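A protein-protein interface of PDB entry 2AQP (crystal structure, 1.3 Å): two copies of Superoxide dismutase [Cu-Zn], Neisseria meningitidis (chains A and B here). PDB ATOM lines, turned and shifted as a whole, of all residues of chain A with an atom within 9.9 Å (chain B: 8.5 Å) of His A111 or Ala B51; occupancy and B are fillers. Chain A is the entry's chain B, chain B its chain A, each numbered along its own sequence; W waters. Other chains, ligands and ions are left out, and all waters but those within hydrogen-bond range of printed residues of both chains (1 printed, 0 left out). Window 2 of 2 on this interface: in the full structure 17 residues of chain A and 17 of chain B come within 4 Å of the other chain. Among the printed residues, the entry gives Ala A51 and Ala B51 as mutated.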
ATOM      1  N   LEU A  46       3.412 -23.698   4.423  1.00  0.00           N
ATOM      2  CA  LEU A  46       4.257 -24.490   3.554  1.00  0.00           C
ATOM      3  C   LEU A  46       5.591 -24.802   4.190  1.00  0.00           C
ATOM      4  O   LEU A  46       6.030 -24.020   5.054  1.00  0.00           O
ATOM      5  CB  LEU A  46       4.500 -23.725   2.247  1.00  0.00           C
ATOM      6  CG  LEU A  46       3.256 -23.403   1.432  1.00  0.00           C
ATOM      7  CD1 LEU A  46       3.556 -22.367   0.336  1.00  0.00           C
ATOM      8  CD2 LEU A  46       2.651 -24.650   0.766  1.00  0.00           C
ATOM      9  N   GLN A  47       6.231 -25.886   3.770  1.00  0.00           N
ATOM     10  CA  GLN A  47       7.593 -26.219   4.210  1.00  0.00           C
ATOM     11  C   GLN A  47       8.342 -26.890   3.074  1.00  0.00           C
ATOM     12  O   GLN A  47       7.717 -27.431   2.155  1.00  0.00           O
ATOM     13  CB  GLN A  47       7.556 -27.091   5.470  1.00  0.00           C
ATOM     14  CG  GLN A  47       6.680 -28.309   5.391  1.00  0.00           C
ATOM     15  CD  GLN A  47       7.336 -29.517   4.788  1.00  0.00           C
ATOM     16  OE1 GLN A  47       8.574 -29.550   4.781  1.00  0.00           O
ATOM     17  NE2 GLN A  47       6.461 -30.401   4.343  1.00  0.00           N
ATOM     18  N   GLY A  48       9.678 -26.856   3.160  1.00  0.00           N
ATOM     19  CA  GLY A  48      10.472 -27.594   2.213  1.00  0.00           C
ATOM     20  C   GLY A  48      10.712 -26.931   0.872  1.00  0.00           C
ATOM     21  O   GLY A  48      11.151 -27.618  -0.054  1.00  0.00           O
ATOM     22  N   LEU A  49      10.419 -25.653   0.778  1.00  0.00           N
ATOM     23  CA  LEU A  49      10.637 -24.890  -0.466  1.00  0.00           C
ATOM     24  C   LEU A  49      11.918 -24.061  -0.398  1.00  0.00           C
ATOM     25  O   LEU A  49      12.409 -23.661   0.643  1.00  0.00           O
ATOM     26  CB  LEU A  49       9.430 -23.984  -0.745  1.00  0.00           C
ATOM     27  CG  LEU A  49       8.127 -24.723  -1.045  1.00  0.00           C
ATOM     28  CD1 LEU A  49       7.028 -23.682  -1.141  1.00  0.00           C
ATOM     29  CD2 LEU A  49       8.192 -25.540  -2.319  1.00  0.00           C
ATOM     30  N   SER A  50      12.495 -23.766  -1.574  1.00  0.00           N
ATOM     31  CA  SER A  50      13.694 -22.927  -1.634  1.00  0.00           C
ATOM     32  C   SER A  50      13.374 -21.529  -1.095  1.00  0.00           C
ATOM     33  O   SER A  50      12.371 -20.897  -1.435  1.00  0.00           O
ATOM     34  CB  SER A  50      14.216 -22.883  -3.067  1.00  0.00           C
ATOM     35  OG  SER A  50      15.463 -22.270  -3.117  1.00  0.00           O
ATOM     36  N   ALA A  51      14.239 -21.017  -0.231  1.00  0.00           N
ATOM     37  CA  ALA A  51      14.058 -19.726   0.407  1.00  0.00           C
ATOM     38  C   ALA A  51      14.092 -18.595  -0.610  1.00  0.00           C
ATOM     39  O   ALA A  51      14.858 -18.620  -1.577  1.00  0.00           O
ATOM     40  CB  ALA A  51      15.131 -19.482   1.467  1.00  0.00           C
ATOM     41  N   GLY A  52      13.288 -17.578  -0.401  1.00  0.00           N
ATOM     42  CA  GLY A  52      13.276 -16.437  -1.285  1.00  0.00           C
ATOM     43  C   GLY A  52      11.880 -15.893  -1.501  1.00  0.00           C
ATOM     44  O   GLY A  52      10.894 -16.419  -1.008  1.00  0.00           O
ATOM     45  N   LEU A  53      11.829 -14.821  -2.285  1.00  0.00           N
ATOM     46  CA  LEU A  53      10.573 -14.215  -2.718  1.00  0.00           C
ATOM     47  C   LEU A  53      10.198 -14.791  -4.066  1.00  0.00           C
ATOM     48  O   LEU A  53      10.976 -14.680  -5.014  1.00  0.00           O
ATOM     49  CB  LEU A  53      10.675 -12.691  -2.731  1.00  0.00           C
ATOM     50  CG  LEU A  53       9.385 -11.942  -3.065  1.00  0.00           C
ATOM     51  CD1 LEU A  53       8.355 -12.145  -1.963  1.00  0.00           C
ATOM     52  CD2 LEU A  53       9.652 -10.463  -3.249  1.00  0.00           C
ATOM     53  N   HIS A  54       9.041 -15.399  -4.180  1.00  0.00           N
ATOM     54  CA  HIS A  54       8.688 -16.189  -5.353  1.00  0.00           C
ATOM     55  C   HIS A  54       7.416 -15.683  -6.007  1.00  0.00           C
ATOM     56  O   HIS A  54       6.438 -15.384  -5.335  1.00  0.00           O
ATOM     57  CB  HIS A  54       8.444 -17.646  -4.963  1.00  0.00           C
ATOM     58  CG  HIS A  54       9.638 -18.361  -4.453  1.00  0.00           C
ATOM     59  ND1 HIS A  54      10.524 -18.959  -5.307  1.00  0.00           N
ATOM     60  CD2 HIS A  54      10.160 -18.538  -3.207  1.00  0.00           C
ATOM     61  CE1 HIS A  54      11.503 -19.485  -4.581  1.00  0.00           C
ATOM     62  NE2 HIS A  54      11.311 -19.271  -3.303  1.00  0.00           N
ATOM     63  N   THR A 108       6.533 -15.021   0.184  1.00  0.00           N
ATOM     64  CA  THR A 108       7.821 -15.027   0.916  1.00  0.00           C
ATOM     65  C   THR A 108       8.062 -16.348   1.566  1.00  0.00           C
ATOM     66  O   THR A 108       7.351 -16.753   2.495  1.00  0.00           O
ATOM     67  CB  THR A 108       7.799 -13.929   2.005  1.00  0.00           C
ATOM     68  OG1 THR A 108       7.583 -12.671   1.337  1.00  0.00           O
ATOM     69  CG2 THR A 108       9.093 -13.886   2.754  1.00  0.00           C
ATOM     70  N   VAL A 109       9.049 -17.093   1.036  1.00  0.00           N
ATOM     71  CA  VAL A 109       9.530 -18.300   1.679  1.00  0.00           C
ATOM     72  C   VAL A 109      10.704 -17.889   2.561  1.00  0.00           C
ATOM     73  O   VAL A 109      11.717 -17.337   2.099  1.00  0.00           O
ATOM     74  CB  VAL A 109       9.926 -19.387   0.664  1.00  0.00           C
ATOM     75  CG1 VAL A 109      10.450 -20.609   1.393  1.00  0.00           C
ATOM     76  CG2 VAL A 109       8.746 -19.757  -0.212  1.00  0.00           C
ATOM     77  N   LEU A 110      10.525 -18.149   3.861  1.00  0.00           N
ATOM     78  CA  LEU A 110      11.494 -17.789   4.886  1.00  0.00           C
ATOM     79  C   LEU A 110      12.782 -18.601   4.730  1.00  0.00           C
ATOM     80  O   LEU A 110      12.870 -19.566   3.962  1.00  0.00           O
ATOM     81  CB  LEU A 110      10.868 -18.008   6.252  1.00  0.00           C
ATOM     82  CG  LEU A 110       9.543 -17.259   6.462  1.00  0.00           C
ATOM     83  CD1 LEU A 110       8.852 -17.839   7.716  1.00  0.00           C
ATOM     84  CD2 LEU A 110       9.745 -15.759   6.563  1.00  0.00           C
ATOM     85  N   HIS A 111      13.810 -18.182   5.445  1.00  0.00           N
ATOM     86  CA  HIS A 111      15.148 -18.729   5.209  1.00  0.00           C
ATOM     87  C   HIS A 111      15.217 -20.229   5.340  1.00  0.00           C
ATOM     88  O   HIS A 111      16.033 -20.847   4.655  1.00  0.00           O
ATOM     89  CB  HIS A 111      16.107 -18.156   6.240  1.00  0.00           C
ATOM     90  CG  HIS A 111      16.192 -16.695   6.445  1.00  0.00           C
ATOM     91  ND1 HIS A 111      16.305 -15.815   5.403  1.00  0.00           N
ATOM     92  CD2 HIS A 111      16.249 -15.913   7.548  1.00  0.00           C
ATOM     93  CE1 HIS A 111      16.391 -14.569   5.827  1.00  0.00           C
ATOM     94  NE2 HIS A 111      16.348 -14.592   7.150  1.00  0.00           N
ATOM     95  N   ASP A 112      14.410 -20.811   6.225  1.00  0.00           N
ATOM     96  CA  ASP A 112      14.417 -22.244   6.478  1.00  0.00           C
ATOM     97  C   ASP A 112      13.511 -23.011   5.539  1.00  0.00           C
ATOM     98  O   ASP A 112      13.350 -24.235   5.730  1.00  0.00           O
ATOM     99  CB  ASP A 112      14.059 -22.587   7.923  1.00  0.00           C
ATOM    100  CG  ASP A 112      12.656 -22.221   8.316  1.00  0.00           C
ATOM    101  OD1 ASP A 112      12.294 -22.532   9.485  1.00  0.00           O
ATOM    102  OD2 ASP A 112      11.912 -21.652   7.476  1.00  0.00           O
ATOM    103  N   GLY A 113      12.898 -22.395   4.534  1.00  0.00           N
ATOM    104  CA  GLY A 113      12.075 -23.080   3.584  1.00  0.00           C
ATOM    105  C   GLY A 113      10.594 -23.138   3.911  1.00  0.00           C
ATOM    106  O   GLY A 113       9.822 -23.741   3.147  1.00  0.00           O
ATOM    107  N   THR A 114      10.168 -22.509   5.000  1.00  0.00           N
ATOM    108  CA  THR A 114       8.769 -22.441   5.354  1.00  0.00           C
ATOM    109  C   THR A 114       8.131 -21.148   4.861  1.00  0.00           C
ATOM    110  O   THR A 114       8.806 -20.171   4.566  1.00  0.00           O
ATOM    111  CB  THR A 114       8.572 -22.537   6.886  1.00  0.00           C
ATOM    112  OG1 THR A 114       9.211 -21.410   7.536  1.00  0.00           O
ATOM    113  CG2 THR A 114       9.177 -23.825   7.440  1.00  0.00           C
ATOM    114  N   ALA A 115       6.801 -21.160   4.762  1.00  0.00           N
ATOM    115  CA  ALA A 115       6.083 -19.953   4.329  1.00  0.00           C
ATOM    116  C   ALA A 115       4.754 -19.920   5.077  1.00  0.00           C
ATOM    117  O   ALA A 115       3.981 -20.867   5.048  1.00  0.00           O
ATOM    118  CB  ALA A 115       5.812 -19.911   2.844  1.00  0.00           C
ATOM    119  N   THR A 116       4.518 -18.824   5.769  1.00  0.00           N
ATOM    120  CA  THR A 116       3.332 -18.552   6.566  1.00  0.00           C
ATOM    121  C   THR A 116       2.730 -17.179   6.358  1.00  0.00           C
ATOM    122  O   THR A 116       1.671 -16.862   6.893  1.00  0.00           O
ATOM    123  CB  THR A 116       3.670 -18.702   8.065  1.00  0.00           C
ATOM    124  OG1 THR A 116       4.692 -17.751   8.421  1.00  0.00           O
ATOM    125  CG2 THR A 116       4.073 -20.146   8.414  1.00  0.00           C
ATOM    126  N   GLY B  48      21.016  -2.692   2.613  1.00  0.00           N
ATOM    127  CA  GLY B  48      21.783  -2.627   3.839  1.00  0.00           C
ATOM    128  C   GLY B  48      21.049  -3.049   5.089  1.00  0.00           C
ATOM    129  O   GLY B  48      21.543  -2.798   6.182  1.00  0.00           O
ATOM    130  N   LEU B  49      19.895  -3.682   4.925  1.00  0.00           N
ATOM    131  CA  LEU B  49      19.108  -4.176   6.058  1.00  0.00           C
ATOM    132  C   LEU B  49      19.271  -5.669   6.238  1.00  0.00           C
ATOM    133  O   LEU B  49      19.555  -6.442   5.330  1.00  0.00           O
ATOM    134  CB  LEU B  49      17.632  -3.825   5.849  1.00  0.00           C
ATOM    135  CG  LEU B  49      17.283  -2.348   5.865  1.00  0.00           C
ATOM    136  CD1 LEU B  49      15.807  -2.198   5.535  1.00  0.00           C
ATOM    137  CD2 LEU B  49      17.600  -1.710   7.202  1.00  0.00           C
ATOM    138  N   SER B  50      19.057  -6.116   7.469  1.00  0.00           N
ATOM    139  CA  SER B  50      19.150  -7.540   7.754  1.00  0.00           C
ATOM    140  C   SER B  50      18.076  -8.286   6.972  1.00  0.00           C
ATOM    141  O   SER B  50      16.903  -7.904   6.935  1.00  0.00           O
ATOM    142  CB  SER B  50      19.071  -7.713   9.279  1.00  0.00           C
ATOM    143  OG  SER B  50      19.354  -9.008   9.664  1.00  0.00           O
ATOM    144  N   ALA B  51      18.457  -9.379   6.331  1.00  0.00           N
ATOM    145  CA  ALA B  51      17.568 -10.176   5.526  1.00  0.00           C
ATOM    146  C   ALA B  51      16.461 -10.838   6.311  1.00  0.00           C
ATOM    147  O   ALA B  51      16.645 -11.320   7.439  1.00  0.00           O
ATOM    148  CB  ALA B  51      18.359 -11.283   4.807  1.00  0.00           C
ATOM    149  N   GLY B  52      15.257 -10.929   5.755  1.00  0.00           N
ATOM    150  CA  GLY B  52      14.171 -11.554   6.470  1.00  0.00           C
ATOM    151  C   GLY B  52      12.848 -10.817   6.197  1.00  0.00           C
ATOM    152  O   GLY B  52      12.803  -9.814   5.510  1.00  0.00           O
ATOM    153  N   LEU B  53      11.791 -11.402   6.748  1.00  0.00           N
ATOM    154  CA  LEU B  53      10.462 -10.811   6.712  1.00  0.00           C
ATOM    155  C   LEU B  53      10.276  -9.966   7.971  1.00  0.00           C
ATOM    156  O   LEU B  53      10.378 -10.520   9.067  1.00  0.00           O
ATOM    157  CB  LEU B  53       9.387 -11.885   6.573  1.00  0.00           C
ATOM    158  CG  LEU B  53       7.981 -11.353   6.427  1.00  0.00           C
ATOM    159  CD1 LEU B  53       7.790 -10.601   5.118  1.00  0.00           C
ATOM    160  CD2 LEU B  53       6.981 -12.511   6.446  1.00  0.00           C
ATOM    161  N   HIS B  54       9.980  -8.692   7.830  1.00  0.00           N
ATOM    162  CA  HIS B  54      10.032  -7.760   8.951  1.00  0.00           C
ATOM    163  C   HIS B  54       8.700  -7.064   9.137  1.00  0.00           C
ATOM    164  O   HIS B  54       8.061  -6.635   8.177  1.00  0.00           O
ATOM    165  CB  HIS B  54      11.068  -6.677   8.695  1.00  0.00           C
ATOM    166  CG  HIS B  54      12.464  -7.191   8.651  1.00  0.00           C
ATOM    167  ND1 HIS B  54      13.211  -7.321   9.805  1.00  0.00           N
ATOM    168  CD2 HIS B  54      13.276  -7.586   7.641  1.00  0.00           C
ATOM    169  CE1 HIS B  54      14.392  -7.789   9.494  1.00  0.00           C
ATOM    170  NE2 HIS B  54      14.467  -7.952   8.198  1.00  0.00           N
ATOM    171  N   LEU B 107       7.261  -6.552   5.401  1.00  0.00           N
ATOM    172  CA  LEU B 107       8.245  -6.130   4.401  1.00  0.00           C
ATOM    173  C   LEU B 107       9.255  -7.241   4.169  1.00  0.00           C
ATOM    174  O   LEU B 107       9.866  -7.749   5.131  1.00  0.00           O
ATOM    175  CB  LEU B 107       8.963  -4.879   4.867  1.00  0.00           C
ATOM    176  CG  LEU B 107      10.081  -4.365   3.969  1.00  0.00           C
ATOM    177  CD1 LEU B 107       9.559  -3.763   2.698  1.00  0.00           C
ATOM    178  CD2 LEU B 107      10.876  -3.299   4.743  1.00  0.00           C
ATOM    179  N   THR B 108       9.453  -7.651   2.909  1.00  0.00           N
ATOM    180  CA  THR B 108      10.436  -8.701   2.586  1.00  0.00           C
ATOM    181  C   THR B 108      11.761  -8.093   2.234  1.00  0.00           C
ATOM    182  O   THR B 108      11.881  -7.444   1.190  1.00  0.00           O
ATOM    183  CB  THR B 108       9.903  -9.559   1.422  1.00  0.00           C
ATOM    184  OG1 THR B 108       8.660 -10.149   1.829  1.00  0.00           O
ATOM    185  CG2 THR B 108      10.875 -10.667   1.059  1.00  0.00           C
ATOM    186  N   VAL B 109      12.753  -8.289   3.133  1.00  0.00           N
ATOM    187  CA  VAL B 109      14.132  -7.939   2.793  1.00  0.00           C
ATOM    188  C   VAL B 109      14.803  -9.183   2.233  1.00  0.00           C
ATOM    189  O   VAL B 109      14.855 -10.215   2.904  1.00  0.00           O
ATOM    190  CB  VAL B 109      14.894  -7.396   4.015  1.00  0.00           C
ATOM    191  CG1 VAL B 109      16.354  -7.092   3.647  1.00  0.00           C
ATOM    192  CG2 VAL B 109      14.182  -6.166   4.560  1.00  0.00           C
ATOM    193  N   LEU B 110      15.274  -9.059   0.994  1.00  0.00           N
ATOM    194  CA  LEU B 110      15.899 -10.147   0.265  1.00  0.00           C
ATOM    195  C   LEU B 110      17.216 -10.566   0.901  1.00  0.00           C
ATOM    196  O   LEU B 110      17.751  -9.884   1.774  1.00  0.00           O
ATOM    197  CB  LEU B 110      16.061  -9.691  -1.202  1.00  0.00           C
ATOM    198  CG  LEU B 110      14.748  -9.240  -1.859  1.00  0.00           C
ATOM    199  CD1 LEU B 110      15.102  -8.505  -3.152  1.00  0.00           C
ATOM    200  CD2 LEU B 110      13.806 -10.395  -2.079  1.00  0.00           C
ATOM    201  N   HIS B 111      17.737 -11.700   0.435  1.00  0.00           N
ATOM    202  CA  HIS B 111      18.865 -12.342   1.110  1.00  0.00           C
ATOM    203  C   HIS B 111      20.037 -11.402   1.234  1.00  0.00           C
ATOM    204  O   HIS B 111      20.789 -11.524   2.198  1.00  0.00           O
ATOM    205  CB  HIS B 111      19.346 -13.505   0.257  1.00  0.00           C
ATOM    206  CG  HIS B 111      18.345 -14.556  -0.054  1.00  0.00           C
ATOM    207  ND1 HIS B 111      17.425 -14.977   0.867  1.00  0.00           N
ATOM    208  CD2 HIS B 111      18.114 -15.308  -1.151  1.00  0.00           C
ATOM    209  CE1 HIS B 111      16.665 -15.936   0.345  1.00  0.00           C
ATOM    210  NE2 HIS B 111      17.058 -16.148  -0.893  1.00  0.00           N
ATOM    211  N   ASP B 112      20.250 -10.529   0.263  1.00  0.00           N
ATOM    212  CA  ASP B 112      21.400  -9.626   0.191  1.00  0.00           C
ATOM    213  C   ASP B 112      21.154  -8.314   0.916  1.00  0.00           C
ATOM    214  O   ASP B 112      22.051  -7.433   0.849  1.00  0.00           O
ATOM    215  CB  ASP B 112      21.843  -9.335  -1.231  1.00  0.00           C
ATOM    216  CG  ASP B 112      20.846  -8.578  -2.073  1.00  0.00           C
ATOM    217  OD1 ASP B 112      21.245  -8.268  -3.221  1.00  0.00           O
ATOM    218  OD2 ASP B 112      19.714  -8.315  -1.566  1.00  0.00           O
ATOM    219  N   GLY B 113      20.037  -8.141   1.602  1.00  0.00           N
ATOM    220  CA  GLY B 113      19.809  -6.933   2.359  1.00  0.00           C
ATOM    221  C   GLY B 113      19.015  -5.877   1.618  1.00  0.00           C
ATOM    222  O   GLY B 113      18.786  -4.815   2.215  1.00  0.00           O
ATOM    223  N   THR B 114      18.601  -6.132   0.392  1.00  0.00           N
ATOM    224  CA  THR B 114      17.832  -5.172  -0.356  1.00  0.00           C
ATOM    225  C   THR B 114      16.348  -5.474  -0.252  1.00  0.00           C
ATOM    226  O   THR B 114      15.920  -6.565   0.089  1.00  0.00           O
ATOM    227  CB  THR B 114      18.214  -5.139  -1.855  1.00  0.00           C
ATOM    228  OG1 THR B 114      17.959  -6.444  -2.429  1.00  0.00           O
ATOM    229  CG2 THR B 114      19.676  -4.742  -2.026  1.00  0.00           C
ATOM    230  N   HIS B 138      10.633  -3.364  11.735  1.00  0.00           N
ATOM    231  CA  HIS B 138      11.062  -4.014  12.938  1.00  0.00           C
ATOM    232  C   HIS B 138      12.135  -5.064  12.713  1.00  0.00           C
ATOM    233  O   HIS B 138      12.261  -5.573  11.604  1.00  0.00           O
ATOM    234  CB  HIS B 138       9.855  -4.643  13.633  1.00  0.00           C
ATOM    235  CG  HIS B 138       8.963  -3.589  14.233  1.00  0.00           C
ATOM    236  ND1 HIS B 138       9.011  -3.182  15.541  1.00  0.00           N
ATOM    237  CD2 HIS B 138       8.001  -2.823  13.644  1.00  0.00           C
ATOM    238  CE1 HIS B 138       8.086  -2.232  15.724  1.00  0.00           C
ATOM    239  NE2 HIS B 138       7.467  -1.995  14.592  1.00  0.00           N
ATOM    240  N   THR B 139      12.819  -5.426  13.786  1.00  0.00           N
ATOM    241  CA  THR B 139      13.767  -6.532  13.662  1.00  0.00           C
ATOM    242  C   THR B 139      13.010  -7.843  13.473  1.00  0.00           C
ATOM    243  O   THR B 139      13.493  -8.674  12.679  1.00  0.00           O
ATOM    244  CB  THR B 139      14.551  -6.518  14.995  1.00  0.00           C
ATOM    245  OG1 THR B 139      15.271  -5.270  15.063  1.00  0.00           O
ATOM    246  CG2 THR B 139      15.539  -7.654  15.116  1.00  0.00           C
ATOM    247  N   MET B 158      14.188  -1.450  13.833  1.00  0.00           N
ATOM    248  CA  MET B 158      15.366  -1.608  13.025  1.00  0.00           C
ATOM    249  C   MET B 158      15.621  -0.420  12.130  1.00  0.00           C
ATOM    250  O   MET B 158      16.747   0.072  11.991  1.00  0.00           O
ATOM    251  CB  MET B 158      15.238  -2.887  12.175  1.00  0.00           C
ATOM    252  CG  MET B 158      16.491  -3.115  11.319  1.00  0.00           C
ATOM    253  SD  MET B 158      16.468  -4.715  10.473  1.00  0.00           S
ATOM    254  CE  MET B 158      15.280  -4.365   9.194  1.00  0.00           C
HETATM  255  O   HOH W   1      18.691 -15.957   3.291  1.00  0.00           O
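Of the 18 printed residues of chain A, 6 touch a printed residue of chain B. Along chain A the printed residues that touch a printed residue of chain B span positions 51 to 111. Of the 18 printed residues of chain B, 6 touch a printed residue of chain A. Hydrophobic or aromatic side chains of chain B within 4 Å of the printed part of chain A: Ala B51, Leu B53, Leu B110 and His B111.
Water W1 bridges ND1 of His B111 (2.9 Å) and ND1 of His A111 (3.2 Å).
Ala A51 touches His B111, and with the chains exchanged His A111 touches Ala B51. Gly A52 touches His B111, and with the chains exchanged His A111 touches Gly B52. Leu A53 touches Leu B110, and with the chains exchanged Leu A110 touches Leu B53. Thr B108 touches its own counterpart, Thr A108. Positions printed for both chains: 48, 49, 50, 51, 52, 53, 54, 108, 109, 110, 111, 112, 113 and 114. Of the 7 pairs that touch across the chains among the printed residues, 7 have their exchanged pair printed and touching as well.
Of the printed residues of chain B, His A111 touches Ala B51 and Gly B52. Of the printed residues of chain A, Ala B51 touches His A111. No residue of chain A comes within 4 Å of Val B109. Printed residues of chain B within 4 Å of Gly A52: His B111. Printed residues of chain B within 4 Å of Ala A51: His B111. Of the printed residues of chain A, Leu B53 touches Leu A110. Of the printed residues of chain B, Thr A108 touches Thr B108. Of the printed residues of chain A, Thr B108 touches Thr A108 (2.8 Å).
NE2 of His B111 is in hydrogen-bond range of O of Ala A51 (3.4 Å). OG1 of Thr B108 lies within hydrogen-bond range of OG1 of Thr A108, at 2.8 Å. NE2 of His A111 is in hydrogen-bond range of O of Ala B51, at 3.3 Å.
The backbone NH (N) of Val A109 is in hydrogen-bond range of the backbone carbonyl oxygen (O) of Gly A52, at 2.8 Å. O of Gly B52 is in hydrogen-bond range of N of Val B109, 2.8 Å away.
CA of Gly A52 touches CE1 of His B111 (3.8 Å). CD2 of Leu B110 touches CB of Leu A53, at 3.9 Å. Leu B53 touches Leu A110 (CB to CD2, 3.9 Å). CA of Gly B52 touches NE2 of His A111, 3.8 Å away.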
